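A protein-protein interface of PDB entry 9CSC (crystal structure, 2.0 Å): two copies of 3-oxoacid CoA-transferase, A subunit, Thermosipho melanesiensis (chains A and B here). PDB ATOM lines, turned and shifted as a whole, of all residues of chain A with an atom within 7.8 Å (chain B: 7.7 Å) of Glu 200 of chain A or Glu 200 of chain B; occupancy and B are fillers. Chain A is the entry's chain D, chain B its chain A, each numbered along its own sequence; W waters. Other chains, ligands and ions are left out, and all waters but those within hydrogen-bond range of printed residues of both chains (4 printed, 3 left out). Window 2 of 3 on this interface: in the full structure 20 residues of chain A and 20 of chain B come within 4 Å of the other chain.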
ATOM      1  N   LYS A 156      16.365 -22.950  -4.697  1.00  0.00           N
ATOM      2  CA  LYS A 156      16.332 -24.194  -5.439  1.00  0.00           C
ATOM      3  C   LYS A 156      17.766 -24.612  -5.732  1.00  0.00           C
ATOM      4  O   LYS A 156      18.636 -23.763  -5.928  1.00  0.00           O
ATOM      5  CB  LYS A 156      15.629 -24.076  -6.798  1.00  0.00           C
ATOM      6  CG  LYS A 156      14.252 -23.458  -6.799  1.00  0.00           C
ATOM      7  CD  LYS A 156      13.842 -23.119  -8.209  1.00  0.00           C
ATOM      8  CE  LYS A 156      12.328 -23.065  -8.418  1.00  0.00           C
ATOM      9  NZ  LYS A 156      11.657 -21.937  -7.693  1.00  0.00           N
ATOM     10  N   LEU A 163      22.697 -23.463  -7.653  1.00  0.00           N
ATOM     11  CA  LEU A 163      21.737 -22.751  -6.833  1.00  0.00           C
ATOM     12  C   LEU A 163      21.270 -21.440  -7.470  1.00  0.00           C
ATOM     13  O   LEU A 163      22.024 -20.761  -8.166  1.00  0.00           O
ATOM     14  CB  LEU A 163      22.316 -22.418  -5.466  1.00  0.00           C
ATOM     15  CG  LEU A 163      23.019 -23.561  -4.721  1.00  0.00           C
ATOM     16  CD1 LEU A 163      23.622 -23.061  -3.356  1.00  0.00           C
ATOM     17  CD2 LEU A 163      22.084 -24.762  -4.487  1.00  0.00           C
ATOM     18  N   VAL A 164      20.042 -21.062  -7.106  1.00  0.00           N
ATOM     19  CA  VAL A 164      19.448 -19.749  -7.339  1.00  0.00           C
ATOM     20  C   VAL A 164      18.825 -19.304  -6.015  1.00  0.00           C
ATOM     21  O   VAL A 164      18.459 -20.116  -5.163  1.00  0.00           O
ATOM     22  CB  VAL A 164      18.395 -19.776  -8.468  1.00  0.00           C
ATOM     23  CG1 VAL A 164      19.011 -20.036  -9.844  1.00  0.00           C
ATOM     24  CG2 VAL A 164      17.324 -20.879  -8.184  1.00  0.00           C
ATOM     25  N   TYR A 165      18.775 -18.017  -5.823  1.00  0.00           N
ATOM     26  CA  TYR A 165      18.260 -17.371  -4.652  1.00  0.00           C
ATOM     27  C   TYR A 165      16.989 -16.636  -5.053  1.00  0.00           C
ATOM     28  O   TYR A 165      16.599 -16.662  -6.211  1.00  0.00           O
ATOM     29  CB  TYR A 165      19.340 -16.463  -4.120  1.00  0.00           C
ATOM     30  CG  TYR A 165      20.629 -17.215  -3.905  1.00  0.00           C
ATOM     31  CD1 TYR A 165      20.845 -17.951  -2.753  1.00  0.00           C
ATOM     32  CD2 TYR A 165      21.628 -17.155  -4.815  1.00  0.00           C
ATOM     33  CE1 TYR A 165      22.035 -18.563  -2.503  1.00  0.00           C
ATOM     34  CE2 TYR A 165      22.819 -17.854  -4.611  1.00  0.00           C
ATOM     35  CZ  TYR A 165      23.005 -18.538  -3.437  1.00  0.00           C
ATOM     36  OH  TYR A 165      24.183 -19.183  -3.193  1.00  0.00           O
ATOM     37  N   GLY A 194      18.730 -28.498 -16.066  1.00  0.00           N
ATOM     38  CA  GLY A 194      18.028 -27.822 -17.152  1.00  0.00           C
ATOM     39  C   GLY A 194      16.836 -26.987 -16.717  1.00  0.00           C
ATOM     40  O   GLY A 194      16.250 -26.282 -17.534  1.00  0.00           O
ATOM     41  N   THR A 195      16.474 -27.016 -15.443  1.00  0.00           N
ATOM     42  CA  THR A 195      15.476 -26.082 -14.937  1.00  0.00           C
ATOM     43  C   THR A 195      16.084 -24.711 -14.640  1.00  0.00           C
ATOM     44  O   THR A 195      15.445 -23.687 -14.911  1.00  0.00           O
ATOM     45  CB  THR A 195      14.815 -26.713 -13.714  1.00  0.00           C
ATOM     46  OG1 THR A 195      14.119 -27.879 -14.174  1.00  0.00           O
ATOM     47  CG2 THR A 195      13.853 -25.779 -13.070  1.00  0.00           C
ATOM     48  N   LEU A 196      17.342 -24.690 -14.164  1.00  0.00           N
ATOM     49  CA  LEU A 196      18.127 -23.482 -13.913  1.00  0.00           C
ATOM     50  C   LEU A 196      18.973 -23.181 -15.144  1.00  0.00           C
ATOM     51  O   LEU A 196      19.886 -23.937 -15.458  1.00  0.00           O
ATOM     52  CB  LEU A 196      19.072 -23.657 -12.708  1.00  0.00           C
ATOM     53  CG  LEU A 196      18.414 -24.317 -11.491  1.00  0.00           C
ATOM     54  CD1 LEU A 196      19.253 -24.467 -10.248  1.00  0.00           C
ATOM     55  CD2 LEU A 196      17.155 -23.505 -11.150  1.00  0.00           C
ATOM     56  N   SER A 197      18.717 -22.055 -15.805  1.00  0.00           N
ATOM     57  CA  SER A 197      19.474 -21.737 -16.995  1.00  0.00           C
ATOM     58  C   SER A 197      20.895 -21.264 -16.670  1.00  0.00           C
ATOM     59  O   SER A 197      21.139 -20.669 -15.608  1.00  0.00           O
ATOM     60  CB  SER A 197      18.738 -20.681 -17.818  1.00  0.00           C
ATOM     61  OG  SER A 197      19.629 -19.892 -18.555  1.00  0.00           O
ATOM     62  N   PRO A 198      21.823 -21.467 -17.600  1.00  0.00           N
ATOM     63  CA  PRO A 198      23.199 -20.990 -17.406  1.00  0.00           C
ATOM     64  C   PRO A 198      23.267 -19.509 -17.088  1.00  0.00           C
ATOM     65  O   PRO A 198      24.130 -19.119 -16.312  1.00  0.00           O
ATOM     66  CB  PRO A 198      23.918 -21.346 -18.720  1.00  0.00           C
ATOM     67  CG  PRO A 198      22.995 -22.355 -19.418  1.00  0.00           C
ATOM     68  CD  PRO A 198      21.618 -21.951 -18.979  1.00  0.00           C
ATOM     69  N   ASN A 199      22.385 -18.676 -17.674  1.00  0.00           N
ATOM     70  CA  ASN A 199      22.331 -17.224 -17.412  1.00  0.00           C
ATOM     71  C   ASN A 199      21.715 -16.857 -16.062  1.00  0.00           C
ATOM     72  O   ASN A 199      21.813 -15.704 -15.641  1.00  0.00           O
ATOM     73  CB  ASN A 199      21.520 -16.508 -18.502  1.00  0.00           C
ATOM     74  CG  ASN A 199      22.149 -16.618 -19.858  1.00  0.00           C
ATOM     75  OD1 ASN A 199      23.333 -16.400 -19.986  1.00  0.00           O
ATOM     76  ND2 ASN A 199      21.367 -16.921 -20.878  1.00  0.00           N
ATOM     77  N   GLU A 200      21.027 -17.788 -15.408  1.00  0.00           N
ATOM     78  CA  GLU A 200      20.348 -17.523 -14.150  1.00  0.00           C
ATOM     79  C   GLU A 200      21.076 -18.007 -12.906  1.00  0.00           C
ATOM     80  O   GLU A 200      20.779 -17.535 -11.807  1.00  0.00           O
ATOM     81  CB  GLU A 200      18.999 -18.245 -14.051  1.00  0.00           C
ATOM     82  CG  GLU A 200      17.905 -17.938 -15.025  1.00  0.00           C
ATOM     83  CD  GLU A 200      16.811 -19.048 -15.052  1.00  0.00           C
ATOM     84  OE1 GLU A 200      15.727 -18.793 -15.586  1.00  0.00           O
ATOM     85  OE2 GLU A 200      16.985 -20.176 -14.569  1.00  0.00           O
ATOM     86  N   ILE A 201      21.854 -19.084 -13.034  1.00  0.00           N
ATOM     87  CA  ILE A 201      22.496 -19.713 -11.885  1.00  0.00           C
ATOM     88  C   ILE A 201      23.410 -18.698 -11.213  1.00  0.00           C
ATOM     89  O   ILE A 201      24.220 -18.036 -11.873  1.00  0.00           O
ATOM     90  CB  ILE A 201      23.300 -20.956 -12.327  1.00  0.00           C
ATOM     91  CG1 ILE A 201      22.387 -22.140 -12.719  1.00  0.00           C
ATOM     92  CG2 ILE A 201      24.335 -21.383 -11.248  1.00  0.00           C
ATOM     93  CD1 ILE A 201      22.974 -23.011 -13.791  1.00  0.00           C
ATOM     94  N   LYS A 202      23.364 -18.643  -9.899  1.00  0.00           N
ATOM     95  CA  LYS A 202      24.242 -17.729  -9.191  1.00  0.00           C
ATOM     96  C   LYS A 202      25.314 -18.414  -8.351  1.00  0.00           C
ATOM     97  O   LYS A 202      26.308 -17.763  -8.027  1.00  0.00           O
ATOM     98  CB  LYS A 202      23.403 -16.784  -8.320  1.00  0.00           C
ATOM     99  CG  LYS A 202      22.615 -15.783  -9.208  1.00  0.00           C
ATOM    100  CD  LYS A 202      21.918 -14.744  -8.373  1.00  0.00           C
ATOM    101  CE  LYS A 202      21.270 -13.622  -9.197  1.00  0.00           C
ATOM    102  NZ  LYS A 202      20.221 -12.806  -8.390  1.00  0.00           N
ATOM    103  N   THR A 203      25.162 -19.693  -7.993  1.00  0.00           N
ATOM    104  CA  THR A 203      26.264 -20.444  -7.392  1.00  0.00           C
ATOM    105  C   THR A 203      26.423 -21.771  -8.135  1.00  0.00           C
ATOM    106  O   THR A 203      25.487 -22.586  -8.143  1.00  0.00           O
ATOM    107  CB  THR A 203      26.019 -20.689  -5.901  1.00  0.00           C
ATOM    108  OG1 THR A 203      25.887 -19.463  -5.178  1.00  0.00           O
ATOM    109  CG2 THR A 203      27.151 -21.529  -5.362  1.00  0.00           C
ATOM    110  N   LYS B 156      19.626  -7.963 -24.004  1.00  0.00           N
ATOM    111  CA  LYS B 156      18.342  -7.281 -23.873  1.00  0.00           C
ATOM    112  C   LYS B 156      18.452  -6.145 -22.850  1.00  0.00           C
ATOM    113  O   LYS B 156      19.219  -6.229 -21.875  1.00  0.00           O
ATOM    114  CB  LYS B 156      17.201  -8.255 -23.445  1.00  0.00           C
ATOM    115  CG  LYS B 156      17.068  -9.533 -24.279  1.00  0.00           C
ATOM    116  CD  LYS B 156      15.943 -10.425 -23.748  1.00  0.00           C
ATOM    117  CE  LYS B 156      15.643 -11.599 -24.659  1.00  0.00           C
ATOM    118  NZ  LYS B 156      15.145 -12.842 -23.921  1.00  0.00           N
ATOM    119  N   LEU B 163      19.533  -4.680 -17.823  1.00  0.00           N
ATOM    120  CA  LEU B 163      20.221  -5.462 -18.840  1.00  0.00           C
ATOM    121  C   LEU B 163      20.398  -6.903 -18.397  1.00  0.00           C
ATOM    122  O   LEU B 163      20.665  -7.167 -17.222  1.00  0.00           O
ATOM    123  CB  LEU B 163      21.605  -4.934 -19.117  1.00  0.00           C
ATOM    124  CG  LEU B 163      21.704  -3.440 -19.385  1.00  0.00           C
ATOM    125  CD1 LEU B 163      23.190  -3.117 -19.729  1.00  0.00           C
ATOM    126  CD2 LEU B 163      20.791  -3.016 -20.552  1.00  0.00           C
ATOM    127  N   VAL B 164      20.306  -7.828 -19.350  1.00  0.00           N
ATOM    128  CA  VAL B 164      20.744  -9.222 -19.184  1.00  0.00           C
ATOM    129  C   VAL B 164      21.740  -9.502 -20.301  1.00  0.00           C
ATOM    130  O   VAL B 164      21.717  -8.845 -21.346  1.00  0.00           O
ATOM    131  CB  VAL B 164      19.632 -10.297 -19.211  1.00  0.00           C
ATOM    132  CG1 VAL B 164      18.786 -10.165 -17.929  1.00  0.00           C
ATOM    133  CG2 VAL B 164      18.827 -10.196 -20.507  1.00  0.00           C
ATOM    134  N   TYR B 165      22.648 -10.443 -20.059  1.00  0.00           N
ATOM    135  CA  TYR B 165      23.693 -10.848 -20.996  1.00  0.00           C
ATOM    136  C   TYR B 165      23.452 -12.307 -21.393  1.00  0.00           C
ATOM    137  O   TYR B 165      22.690 -13.038 -20.740  1.00  0.00           O
ATOM    138  CB  TYR B 165      25.108 -10.663 -20.379  1.00  0.00           C
ATOM    139  CG  TYR B 165      25.366  -9.252 -19.868  1.00  0.00           C
ATOM    140  CD1 TYR B 165      24.998  -8.881 -18.576  1.00  0.00           C
ATOM    141  CD2 TYR B 165      25.940  -8.279 -20.677  1.00  0.00           C
ATOM    142  CE1 TYR B 165      25.201  -7.593 -18.103  1.00  0.00           C
ATOM    143  CE2 TYR B 165      26.124  -6.954 -20.210  1.00  0.00           C
ATOM    144  CZ  TYR B 165      25.755  -6.646 -18.933  1.00  0.00           C
ATOM    145  OH  TYR B 165      25.934  -5.403 -18.461  1.00  0.00           O
ATOM    146  N   GLY B 194       9.249  -6.008 -16.871  1.00  0.00           N
ATOM    147  CA  GLY B 194       8.601  -7.202 -16.415  1.00  0.00           C
ATOM    148  C   GLY B 194       8.943  -8.438 -17.186  1.00  0.00           C
ATOM    149  O   GLY B 194       8.589  -9.525 -16.732  1.00  0.00           O
ATOM    150  N   THR B 195       9.616  -8.301 -18.328  1.00  0.00           N
ATOM    151  CA  THR B 195      10.152  -9.438 -19.064  1.00  0.00           C
ATOM    152  C   THR B 195      11.379  -9.992 -18.353  1.00  0.00           C
ATOM    153  O   THR B 195      11.537 -11.209 -18.240  1.00  0.00           O
ATOM    154  CB  THR B 195      10.489  -9.013 -20.506  1.00  0.00           C
ATOM    155  OG1 THR B 195       9.296  -8.567 -21.152  1.00  0.00           O
ATOM    156  CG2 THR B 195      11.043 -10.149 -21.297  1.00  0.00           C
ATOM    157  N   LEU B 196      12.243  -9.112 -17.849  1.00  0.00           N
ATOM    158  CA  LEU B 196      13.409  -9.502 -17.075  1.00  0.00           C
ATOM    159  C   LEU B 196      13.096  -9.429 -15.590  1.00  0.00           C
ATOM    160  O   LEU B 196      12.754  -8.360 -15.070  1.00  0.00           O
ATOM    161  CB  LEU B 196      14.591  -8.595 -17.397  1.00  0.00           C
ATOM    162  CG  LEU B 196      14.831  -8.271 -18.860  1.00  0.00           C
ATOM    163  CD1 LEU B 196      15.962  -7.205 -18.964  1.00  0.00           C
ATOM    164  CD2 LEU B 196      15.173  -9.476 -19.719  1.00  0.00           C
ATOM    165  N   SER B 197      13.233 -10.561 -14.925  1.00  0.00           N
ATOM    166  CA  SER B 197      12.936 -10.736 -13.531  1.00  0.00           C
ATOM    167  C   SER B 197      13.936 -10.037 -12.617  1.00  0.00           C
ATOM    168  O   SER B 197      15.125 -10.015 -12.882  1.00  0.00           O
ATOM    169  CB  SER B 197      12.969 -12.227 -13.219  1.00  0.00           C
ATOM    170  OG  SER B 197      12.817 -12.523 -11.847  1.00  0.00           O
ATOM    171  N   PRO B 198      13.504  -9.663 -11.437  1.00  0.00           N
ATOM    172  CA  PRO B 198      14.470  -9.108 -10.480  1.00  0.00           C
ATOM    173  C   PRO B 198      15.603 -10.097 -10.187  1.00  0.00           C
ATOM    174  O   PRO B 198      16.709  -9.670  -9.844  1.00  0.00           O
ATOM    175  CB  PRO B 198      13.623  -8.816  -9.238  1.00  0.00           C
ATOM    176  CG  PRO B 198      12.172  -8.795  -9.722  1.00  0.00           C
ATOM    177  CD  PRO B 198      12.146  -9.781 -10.890  1.00  0.00           C
ATOM    178  N   ASN B 199      15.327 -11.410 -10.271  1.00  0.00           N
ATOM    179  CA  ASN B 199      16.334 -12.430  -9.999  1.00  0.00           C
ATOM    180  C   ASN B 199      17.296 -12.673 -11.153  1.00  0.00           C
ATOM    181  O   ASN B 199      18.346 -13.255 -10.909  1.00  0.00           O
ATOM    182  CB  ASN B 199      15.656 -13.768  -9.601  1.00  0.00           C
ATOM    183  CG  ASN B 199      14.950 -13.694  -8.231  1.00  0.00           C
ATOM    184  OD1 ASN B 199      15.509 -13.207  -7.253  1.00  0.00           O
ATOM    185  ND2 ASN B 199      13.676 -14.100  -8.191  1.00  0.00           N
ATOM    186  N   GLU B 200      17.021 -12.132 -12.357  1.00  0.00           N
ATOM    187  CA  GLU B 200      17.795 -12.381 -13.570  1.00  0.00           C
ATOM    188  C   GLU B 200      18.616 -11.207 -14.074  1.00  0.00           C
ATOM    189  O   GLU B 200      19.622 -11.419 -14.741  1.00  0.00           O
ATOM    190  CB  GLU B 200      16.858 -12.768 -14.726  1.00  0.00           C
ATOM    191  CG  GLU B 200      16.320 -14.174 -14.762  1.00  0.00           C
ATOM    192  CD  GLU B 200      14.925 -14.253 -15.454  1.00  0.00           C
ATOM    193  OE1 GLU B 200      14.607 -13.371 -16.321  1.00  0.00           O
ATOM    194  OE2 GLU B 200      14.161 -15.213 -15.140  1.00  0.00           O
ATOM    195  N   ILE B 201      18.178  -9.978 -13.833  1.00  0.00           N
ATOM    196  CA  ILE B 201      18.894  -8.818 -14.332  1.00  0.00           C
ATOM    197  C   ILE B 201      20.297  -8.822 -13.768  1.00  0.00           C
ATOM    198  O   ILE B 201      20.482  -9.101 -12.586  1.00  0.00           O
ATOM    199  CB  ILE B 201      18.149  -7.545 -13.881  1.00  0.00           C
ATOM    200  CG1 ILE B 201      16.807  -7.437 -14.603  1.00  0.00           C
ATOM    201  CG2 ILE B 201      19.047  -6.341 -13.985  1.00  0.00           C
ATOM    202  CD1 ILE B 201      15.752  -6.736 -13.796  1.00  0.00           C
ATOM    203  N   LYS B 202      21.284  -8.420 -14.574  1.00  0.00           N
ATOM    204  CA  LYS B 202      22.675  -8.350 -14.102  1.00  0.00           C
ATOM    205  C   LYS B 202      23.212  -6.938 -13.980  1.00  0.00           C
ATOM    206  O   LYS B 202      24.151  -6.702 -13.212  1.00  0.00           O
ATOM    207  CB  LYS B 202      23.587  -9.195 -15.007  1.00  0.00           C
ATOM    208  CG  LYS B 202      23.271 -10.682 -14.780  1.00  0.00           C
ATOM    209  CD  LYS B 202      24.246 -11.697 -15.382  1.00  0.00           C
ATOM    210  CE  LYS B 202      24.033 -13.123 -14.784  1.00  0.00           C
ATOM    211  NZ  LYS B 202      24.637 -14.219 -15.644  1.00  0.00           N
ATOM    212  N   THR B 203      22.616  -5.991 -14.684  1.00  0.00           N
ATOM    213  CA  THR B 203      23.026  -4.604 -14.595  1.00  0.00           C
ATOM    214  C   THR B 203      21.775  -3.745 -14.458  1.00  0.00           C
ATOM    215  O   THR B 203      20.887  -3.816 -15.337  1.00  0.00           O
ATOM    216  CB  THR B 203      23.841  -4.239 -15.820  1.00  0.00           C
ATOM    217  OG1 THR B 203      25.044  -5.028 -15.930  1.00  0.00           O
ATOM    218  CG2 THR B 203      24.230  -2.761 -15.730  1.00  0.00           C
HETATM  219  O   HOH W   1      20.245 -13.213 -16.330  1.00  0.00           O
HETATM  220  O   HOH W   2      14.643 -17.333  -7.837  1.00  0.00           O
HETATM  221  O   HOH W   3      24.054 -14.179 -18.674  1.00  0.00           O
HETATM  222  O   HOH W   4      17.952 -13.626  -7.329  1.00  0.00           O
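Among the printed residues, pairs that only touch across the chains: Asn 199 of chain A with Tyr 165 of chain B (3.5 Å), Tyr 165 of chain A with Asn 199 of chain B (3.8 Å) and Glu 200 of chain A with Glu 200 of chain B (3.9 Å).
Glu 200 of chain A touches just one residue of chain B: Glu 200. Of chain A, only Glu 200 (3.9 Å) comes within 4 Å of Glu 200 of chain B. Of the printed residues of chain A, Asn 199 of chain B touches Tyr 165 (3.8 Å) and Lys 202 (3.2 Å). Of the printed residues of chain A, Lys 202 of chain B touches Asn 199 (3.2 Å). Of the printed residues of chain B, Lys 202 of chain A touches Asn 199. The nearest residue of chain B that does not touch Glu 200 of chain A is Asn 199 of chain B (5.0 Å). The nearest printed residue of chain A that does not touch Asn 199 of chain B is Glu 200 of chain A (5.0 Å).
The backbone carbonyl oxygen of Asn 199 of chain B sits at hydrogen-bond distance from the side-chain amino group of Lys 202 of chain A (3.2 Å). The side-chain amino group (NZ) of Lys 202 of chain B sits at hydrogen-bond distance from the backbone carbonyl oxygen (O) of Asn 199 of chain A, at 3.2 Å.
Tyr 165 of chain A touches Asn 199 of chain B, and with the chains exchanged Asn 199 of chain A touches Tyr 165 of chain B. Asn 199 of chain A touches Lys 202 of chain B, and with the chains exchanged Lys 202 of chain A touches Asn 199 of chain B. Glu 200 of chain A touches its own counterpart, Glu 200 of chain B.
Water W1 bridges the backbone carbonyl oxygen of Glu 200 of chain B and the backbone carbonyl oxygen of Asn 199 of chain A. Water W4 lies within hydrogen-bond range of OD1 of Asn 199 of chain B (2.5 Å) and NZ of Lys 202 of chain A (2.6 Å). Water W2 lies within hydrogen-bond range of the backbone carbonyl oxygen (O) of Tyr 165 of chain A (2.6 Å) and the side-chain amide nitrogen (ND2) of Asn 199 of chain B (3.4 Å). Water W3 lies within hydrogen-bond range of the side-chain amide oxygen of Asn 199 of chain A (2.7 Å), the backbone carbonyl oxygen of Tyr 165 of chain B (2.7 Å) and the side-chain amino group of Lys 202 of chain B (3.1 Å).
Of the 14 printed residues of chain B, 4 touch a printed residue of chain A. Of the 14 printed residues of chain A, 4 touch a printed residue of chain B.
OE2 of Glu 200 of chain A is in hydrogen-bond range of N of Ser 197 of chain A, 2.8 Å away. The side-chain hydroxyl of Thr 203 of chain A is in hydrogen-bond range of the side-chain hydroxyl of Tyr 165 of chain A (2.6 Å). The backbone carbonyl oxygen of Leu 163 of chain B is in hydrogen-bond range of the backbone NH of Lys 202 of chain B (3.0 Å). The backbone NH of Asn 199 of chain B lies close to the side-chain hydroxyl of Ser 197 of chain B, 3.2 Å away. OG1 of Thr 203 of chain B sits at hydrogen-bond distance from OH of Tyr 165 of chain B, at 2.7 Å. N of Asn 199 of chain A sits at hydrogen-bond distance from OG of Ser 197 of chain A (3.1 Å).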
